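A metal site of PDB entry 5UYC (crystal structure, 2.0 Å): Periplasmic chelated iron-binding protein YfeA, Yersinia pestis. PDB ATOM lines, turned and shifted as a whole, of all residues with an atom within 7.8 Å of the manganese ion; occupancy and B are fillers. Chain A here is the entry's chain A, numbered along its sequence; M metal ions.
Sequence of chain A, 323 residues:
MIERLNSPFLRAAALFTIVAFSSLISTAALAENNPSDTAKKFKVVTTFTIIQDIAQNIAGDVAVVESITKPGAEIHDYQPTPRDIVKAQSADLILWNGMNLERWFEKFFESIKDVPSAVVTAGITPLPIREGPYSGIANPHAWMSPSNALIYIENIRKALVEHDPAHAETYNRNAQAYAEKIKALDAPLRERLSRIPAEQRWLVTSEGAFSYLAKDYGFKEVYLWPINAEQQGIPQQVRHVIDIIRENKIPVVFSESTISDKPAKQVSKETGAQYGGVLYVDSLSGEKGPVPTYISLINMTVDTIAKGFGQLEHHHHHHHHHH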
ATOM      1  N   GLU A  74      24.913  11.152  -5.263  1.00  0.00           N
ATOM      2  CA  GLU A  74      23.821  11.088  -6.234  1.00  0.00           C
ATOM      3  C   GLU A  74      24.113  12.020  -7.407  1.00  0.00           C
ATOM      4  O   GLU A  74      24.340  13.215  -7.211  1.00  0.00           O
ATOM      5  CB  GLU A  74      22.520  11.466  -5.523  1.00  0.00           C
ATOM      6  CG  GLU A  74      21.265  10.959  -6.210  1.00  0.00           C
ATOM      7  CD  GLU A  74      21.047  11.652  -7.521  1.00  0.00           C
ATOM      8  OE1 GLU A  74      20.925  12.907  -7.516  1.00  0.00           O
ATOM      9  OE2 GLU A  74      21.015  10.942  -8.566  1.00  0.00           O
ATOM     10  N   ILE A  75      24.112  11.471  -8.631  1.00  0.00           N
ATOM     11  CA  ILE A  75      24.635  12.203  -9.775  1.00  0.00           C
ATOM     12  C   ILE A  75      23.594  12.977 -10.588  1.00  0.00           C
ATOM     13  O   ILE A  75      23.970  13.910 -11.310  1.00  0.00           O
ATOM     14  CB  ILE A  75      25.403  11.255 -10.718  1.00  0.00           C
ATOM     15  CG1 ILE A  75      24.448  10.234 -11.362  1.00  0.00           C
ATOM     16  CG2 ILE A  75      26.513  10.555  -9.957  1.00  0.00           C
ATOM     17  CD1 ILE A  75      25.135   9.311 -12.367  1.00  0.00           C
ATOM     18  N   HIS A  76      22.318  12.601 -10.514  1.00  0.00           N
ATOM     19  CA  HIS A  76      21.321  13.209 -11.392  1.00  0.00           C
ATOM     20  C   HIS A  76      21.051  14.656 -10.975  1.00  0.00           C
ATOM     21  O   HIS A  76      21.048  15.570 -11.816  1.00  0.00           O
ATOM     22  CB  HIS A  76      20.021  12.399 -11.357  1.00  0.00           C
ATOM     23  CG  HIS A  76      20.146  11.004 -11.899  1.00  0.00           C
ATOM     24  ND1 HIS A  76      19.589  10.630 -13.104  1.00  0.00           N
ATOM     25  CD2 HIS A  76      20.729   9.898 -11.396  1.00  0.00           C
ATOM     26  CE1 HIS A  76      19.841   9.346 -13.322  1.00  0.00           C
ATOM     27  NE2 HIS A  76      20.521   8.868 -12.293  1.00  0.00           N
ATOM     28  N   LEU A 101      21.278  12.859 -18.217  1.00  0.00           N
ATOM     29  CA  LEU A 101      21.781  12.344 -16.946  1.00  0.00           C
ATOM     30  C   LEU A 101      22.002  13.501 -15.967  1.00  0.00           C
ATOM     31  O   LEU A 101      21.325  13.604 -14.942  1.00  0.00           O
ATOM     32  CB  LEU A 101      23.078  11.551 -17.147  1.00  0.00           C
ATOM     33  CG  LEU A 101      23.693  11.031 -15.837  1.00  0.00           C
ATOM     34  CD1 LEU A 101      22.806  10.002 -15.136  1.00  0.00           C
ATOM     35  CD2 LEU A 101      25.065  10.453 -16.093  1.00  0.00           C
ATOM     36  N   ASN A 139      16.523   7.398 -21.510  1.00  0.00           N
ATOM     37  CA  ASN A 139      17.069   6.864 -20.273  1.00  0.00           C
ATOM     38  C   ASN A 139      18.586   7.072 -20.311  1.00  0.00           C
ATOM     39  O   ASN A 139      19.233   6.641 -21.281  1.00  0.00           O
ATOM     40  CB  ASN A 139      16.696   5.386 -20.147  1.00  0.00           C
ATOM     41  CG  ASN A 139      17.081   4.788 -18.803  1.00  0.00           C
ATOM     42  OD1 ASN A 139      18.144   5.087 -18.255  1.00  0.00           O
ATOM     43  ND2 ASN A 139      16.220   3.905 -18.284  1.00  0.00           N
ATOM     44  N   PRO A 140      19.205   7.741 -19.322  1.00  0.00           N
ATOM     45  CA  PRO A 140      20.648   8.034 -19.423  1.00  0.00           C
ATOM     46  C   PRO A 140      21.575   6.847 -19.174  1.00  0.00           C
ATOM     47  O   PRO A 140      22.762   6.937 -19.527  1.00  0.00           O
ATOM     48  CB  PRO A 140      20.859   9.110 -18.360  1.00  0.00           C
ATOM     49  CG  PRO A 140      19.859   8.787 -17.292  1.00  0.00           C
ATOM     50  CD  PRO A 140      18.613   8.354 -18.116  1.00  0.00           C
ATOM     51  N   HIS A 141      21.097   5.774 -18.545  1.00  0.00           N
ATOM     52  CA  HIS A 141      21.997   4.767 -17.981  1.00  0.00           C
ATOM     53  C   HIS A 141      22.529   3.791 -19.032  1.00  0.00           C
ATOM     54  O   HIS A 141      22.543   2.581 -18.792  1.00  0.00           O
ATOM     55  CB  HIS A 141      21.305   3.987 -16.858  1.00  0.00           C
ATOM     56  CG  HIS A 141      20.775   4.857 -15.768  1.00  0.00           C
ATOM     57  ND1 HIS A 141      19.504   5.375 -15.772  1.00  0.00           N
ATOM     58  CD2 HIS A 141      21.369   5.313 -14.629  1.00  0.00           C
ATOM     59  CE1 HIS A 141      19.319   6.107 -14.685  1.00  0.00           C
ATOM     60  NE2 HIS A 141      20.433   6.074 -13.971  1.00  0.00           N
ATOM     61  N   TRP A 143      25.476   3.074 -20.081  1.00  0.00           N
ATOM     62  CA  TRP A 143      26.723   2.359 -19.789  1.00  0.00           C
ATOM     63  C   TRP A 143      26.496   0.971 -19.177  1.00  0.00           C
ATOM     64  O   TRP A 143      27.459   0.201 -19.096  1.00  0.00           O
ATOM     65  CB  TRP A 143      27.596   3.209 -18.842  1.00  0.00           C
ATOM     66  CG  TRP A 143      26.965   3.493 -17.527  1.00  0.00           C
ATOM     67  CD1 TRP A 143      26.999   2.687 -16.414  1.00  0.00           C
ATOM     68  CD2 TRP A 143      26.201   4.653 -17.160  1.00  0.00           C
ATOM     69  NE1 TRP A 143      26.306   3.275 -15.390  1.00  0.00           N
ATOM     70  CE2 TRP A 143      25.797   4.478 -15.814  1.00  0.00           C
ATOM     71  CE3 TRP A 143      25.798   5.813 -17.842  1.00  0.00           C
ATOM     72  CZ2 TRP A 143      25.044   5.441 -15.121  1.00  0.00           C
ATOM     73  CZ3 TRP A 143      25.026   6.764 -17.156  1.00  0.00           C
ATOM     74  CH2 TRP A 143      24.661   6.565 -15.808  1.00  0.00           C
ATOM     75  N   GLU A 207      15.617   2.636  -8.486  1.00  0.00           N
ATOM     76  CA  GLU A 207      15.590   3.426  -9.716  1.00  0.00           C
ATOM     77  C   GLU A 207      15.495   2.482 -10.913  1.00  0.00           C
ATOM     78  O   GLU A 207      16.080   1.395 -10.907  1.00  0.00           O
ATOM     79  CB  GLU A 207      16.843   4.311  -9.835  1.00  0.00           C
ATOM     80  CG  GLU A 207      16.833   5.205 -11.093  1.00  0.00           C
ATOM     81  CD  GLU A 207      18.071   6.087 -11.269  1.00  0.00           C
ATOM     82  OE1 GLU A 207      19.190   5.676 -10.887  1.00  0.00           O
ATOM     83  OE2 GLU A 207      17.925   7.203 -11.821  1.00  0.00           O
ATOM     84  N   GLY A 208      14.759   2.917 -11.944  1.00  0.00           N
ATOM     85  CA  GLY A 208      14.724   2.197 -13.212  1.00  0.00           C
ATOM     86  C   GLY A 208      15.963   2.448 -14.050  1.00  0.00           C
ATOM     87  O   GLY A 208      15.888   2.852 -15.214  1.00  0.00           O
ATOM     88  N   ALA A 209      17.118   2.197 -13.449  1.00  0.00           N
ATOM     89  CA  ALA A 209      18.413   2.503 -14.031  1.00  0.00           C
ATOM     90  C   ALA A 209      18.964   1.357 -14.847  1.00  0.00           C
ATOM     91  O   ALA A 209      20.069   1.480 -15.392  1.00  0.00           O
ATOM     92  CB  ALA A 209      19.413   2.835 -12.903  1.00  0.00           C
ATOM     93  N   PHE A 210      18.257   0.239 -14.930  1.00  0.00           N
ATOM     94  CA  PHE A 210      18.842  -0.961 -15.499  1.00  0.00           C
ATOM     95  C   PHE A 210      18.246  -1.336 -16.854  1.00  0.00           C
ATOM     96  O   PHE A 210      18.511  -2.431 -17.358  1.00  0.00           O
ATOM     97  CB  PHE A 210      18.719  -2.099 -14.480  1.00  0.00           C
ATOM     98  CG  PHE A 210      19.456  -1.795 -13.204  1.00  0.00           C
ATOM     99  CD1 PHE A 210      20.807  -2.043 -13.108  1.00  0.00           C
ATOM    100  CD2 PHE A 210      18.796  -1.170 -12.139  1.00  0.00           C
ATOM    101  CE1 PHE A 210      21.517  -1.713 -11.917  1.00  0.00           C
ATOM    102  CE2 PHE A 210      19.480  -0.851 -10.976  1.00  0.00           C
ATOM    103  CZ  PHE A 210      20.845  -1.107 -10.862  1.00  0.00           C
ATOM    104  N   TRP A 225      10.946   3.853  -8.900  1.00  0.00           N
ATOM    105  CA  TRP A 225      10.799   5.145  -9.563  1.00  0.00           C
ATOM    106  C   TRP A 225      11.574   5.124 -10.872  1.00  0.00           C
ATOM    107  O   TRP A 225      12.645   4.497 -10.935  1.00  0.00           O
ATOM    108  CB  TRP A 225      11.259   6.337  -8.696  1.00  0.00           C
ATOM    109  CG  TRP A 225      12.655   6.229  -8.136  1.00  0.00           C
ATOM    110  CD1 TRP A 225      13.817   6.668  -8.715  1.00  0.00           C
ATOM    111  CD2 TRP A 225      13.015   5.677  -6.858  1.00  0.00           C
ATOM    112  NE1 TRP A 225      14.879   6.411  -7.878  1.00  0.00           N
ATOM    113  CE2 TRP A 225      14.416   5.797  -6.737  1.00  0.00           C
ATOM    114  CE3 TRP A 225      12.289   5.092  -5.821  1.00  0.00           C
ATOM    115  CZ2 TRP A 225      15.109   5.355  -5.604  1.00  0.00           C
ATOM    116  CZ3 TRP A 225      12.975   4.648  -4.696  1.00  0.00           C
ATOM    117  CH2 TRP A 225      14.371   4.788  -4.605  1.00  0.00           C
ATOM    118  N   PRO A 226      11.064   5.753 -11.935  1.00  0.00           N
ATOM    119  CA  PRO A 226      11.708   5.603 -13.255  1.00  0.00           C
ATOM    120  C   PRO A 226      13.090   6.221 -13.352  1.00  0.00           C
ATOM    121  O   PRO A 226      13.946   5.653 -14.052  1.00  0.00           O
ATOM    122  CB  PRO A 226      10.711   6.293 -14.208  1.00  0.00           C
ATOM    123  CG  PRO A 226       9.846   7.150 -13.338  1.00  0.00           C
ATOM    124  CD  PRO A 226       9.784   6.490 -12.002  1.00  0.00           C
ATOM    125  N   ILE A 227      13.350   7.342 -12.685  1.00  0.00           N
ATOM    126  CA  ILE A 227      14.653   8.001 -12.707  1.00  0.00           C
ATOM    127  C   ILE A 227      14.756   8.864 -11.458  1.00  0.00           C
ATOM    128  O   ILE A 227      13.770   9.447 -10.999  1.00  0.00           O
ATOM    129  CB  ILE A 227      14.871   8.815 -14.008  1.00  0.00           C
ATOM    130  CG1 ILE A 227      16.284   9.418 -14.070  1.00  0.00           C
ATOM    131  CG2 ILE A 227      13.837   9.928 -14.153  1.00  0.00           C
ATOM    132  CD1 ILE A 227      16.664   9.896 -15.483  1.00  0.00           C
ATOM    133  N   ASN A 228      15.954   8.913 -10.884  1.00  0.00           N
ATOM    134  CA  ASN A 228      16.199   9.725  -9.694  1.00  0.00           C
ATOM    135  C   ASN A 228      15.690  11.146  -9.916  1.00  0.00           C
ATOM    136  O   ASN A 228      16.007  11.779 -10.925  1.00  0.00           O
ATOM    137  CB  ASN A 228      17.696   9.727  -9.345  1.00  0.00           C
ATOM    138  CG  ASN A 228      18.177   8.384  -8.825  1.00  0.00           C
ATOM    139  OD1 ASN A 228      17.404   7.431  -8.707  1.00  0.00           O
ATOM    140  ND2 ASN A 228      19.465   8.308  -8.505  1.00  0.00           N
ATOM    141  N   GLU A 256      20.157   0.440  -4.980  1.00  0.00           N
ATOM    142  CA  GLU A 256      21.362   0.876  -5.670  1.00  0.00           C
ATOM    143  C   GLU A 256      22.173   1.783  -4.757  1.00  0.00           C
ATOM    144  O   GLU A 256      21.661   2.340  -3.793  1.00  0.00           O
ATOM    145  CB  GLU A 256      21.023   1.596  -6.991  1.00  0.00           C
ATOM    146  CG  GLU A 256      20.144   0.753  -7.935  1.00  0.00           C
ATOM    147  CD  GLU A 256      18.655   0.895  -7.629  1.00  0.00           C
ATOM    148  OE1 GLU A 256      18.170   2.035  -7.564  1.00  0.00           O
ATOM    149  OE2 GLU A 256      17.970  -0.138  -7.435  1.00  0.00           O
ATOM    150  N   THR A 258      23.706   4.724  -4.604  1.00  0.00           N
ATOM    151  CA  THR A 258      23.644   6.151  -4.294  1.00  0.00           C
ATOM    152  C   THR A 258      22.294   6.610  -3.754  1.00  0.00           C
ATOM    153  O   THR A 258      22.098   7.813  -3.558  1.00  0.00           O
ATOM    154  CB  THR A 258      23.987   7.010  -5.516  1.00  0.00           C
ATOM    155  OG1 THR A 258      22.904   6.968  -6.461  1.00  0.00           O
ATOM    156  CG2 THR A 258      25.280   6.549  -6.173  1.00  0.00           C
ATOM    157  N   ILE A 259      21.354   5.701  -3.508  1.00  0.00           N
ATOM    158  CA  ILE A 259      20.038   6.051  -3.031  1.00  0.00           C
ATOM    159  C   ILE A 259      19.725   5.199  -1.797  1.00  0.00           C
ATOM    160  O   ILE A 259      20.505   4.317  -1.425  1.00  0.00           O
ATOM    161  CB  ILE A 259      18.955   5.890  -4.117  1.00  0.00           C
ATOM    162  CG1 ILE A 259      19.091   4.534  -4.843  1.00  0.00           C
ATOM    163  CG2 ILE A 259      19.050   7.018  -5.134  1.00  0.00           C
ATOM    164  CD1 ILE A 259      18.426   3.374  -4.101  1.00  0.00           C
ATOM    165  N   VAL A 281      25.303   1.227 -10.213  1.00  0.00           N
ATOM    166  CA  VAL A 281      24.996   1.749 -11.544  1.00  0.00           C
ATOM    167  C   VAL A 281      25.429   3.221 -11.667  1.00  0.00           C
ATOM    168  O   VAL A 281      26.106   3.592 -12.632  1.00  0.00           O
ATOM    169  CB  VAL A 281      23.503   1.583 -11.876  1.00  0.00           C
ATOM    170  CG1 VAL A 281      22.592   2.044 -10.737  1.00  0.00           C
ATOM    171  CG2 VAL A 281      23.159   2.331 -13.175  1.00  0.00           C
ATOM    172  N   ASP A 282      25.040   4.055 -10.713  1.00  0.00           N
ATOM    173  CA  ASP A 282      25.320   5.481 -10.828  1.00  0.00           C
ATOM    174  C   ASP A 282      26.688   5.876 -10.307  1.00  0.00           C
ATOM    175  O   ASP A 282      27.145   6.993 -10.575  1.00  0.00           O
ATOM    176  CB  ASP A 282      24.258   6.295 -10.084  1.00  0.00           C
ATOM    177  CG  ASP A 282      22.926   6.399 -10.848  1.00  0.00           C
ATOM    178  OD1 ASP A 282      22.801   5.807 -11.937  1.00  0.00           O
ATOM    179  OD2 ASP A 282      22.031   7.093 -10.347  1.00  0.00           O
ATOM    180  N   SER A 283      27.369   5.000  -9.570  1.00  0.00           N
ATOM    181  CA  SER A 283      28.672   5.372  -9.022  1.00  0.00           C
ATOM    182  C   SER A 283      29.513   4.125  -8.796  1.00  0.00           C
ATOM    183  O   SER A 283      28.990   3.042  -8.480  1.00  0.00           O
ATOM    184  CB  SER A 283      28.532   6.140  -7.690  1.00  0.00           C
ATOM    185  OG  SER A 283      29.817   6.421  -7.117  1.00  0.00           O
HETATM  186 MN    MN M   1      20.571   6.861 -11.964  1.00  0.00          MN
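N of His 76 lies within hydrogen-bond range of OE2 of Glu 74 (2.9 Å).
The side-chain carboxylate (OE2) of Glu 207 sits close to the backbone NH (N) of Asn 228 (2.8 Å).
OE1 of Glu 256 lies within hydrogen-bond range of N of Glu 207 (2.8 Å).
A ring nitrogen (ND1) of His 141 sits at hydrogen-bond distance from the side-chain amide oxygen of Asn 139 (2.8 Å).
The side-chain amide nitrogen of Asn 228 lies close to the side-chain carboxylate of Asp 282.
The side-chain amide nitrogen of Asn 228 lies within hydrogen-bond range of the side-chain carboxylate of Glu 74, 3.1 Å away.
The indole nitrogen of Trp 225 is in hydrogen-bond range of the side-chain amide oxygen of Asn 228, 2.8 Å away.
ND2 of Asn 228 touches the manganese ion, at 3.9 Å.
Within 4 Å of the manganese ion: His 76, His 141, Glu 207, Asn 228 and Asp 282.
The manganese ion is bound by NE2 of His 76 (2.0 Å), OE1 of Glu 207 (2.1 Å), NE2 of His 141 (2.2 Å), OD2 of Asp 282 (2.2 Å), OD1 of Asp 282 (2.5 Å) and OE2 of Glu 207 (2.7 Å).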
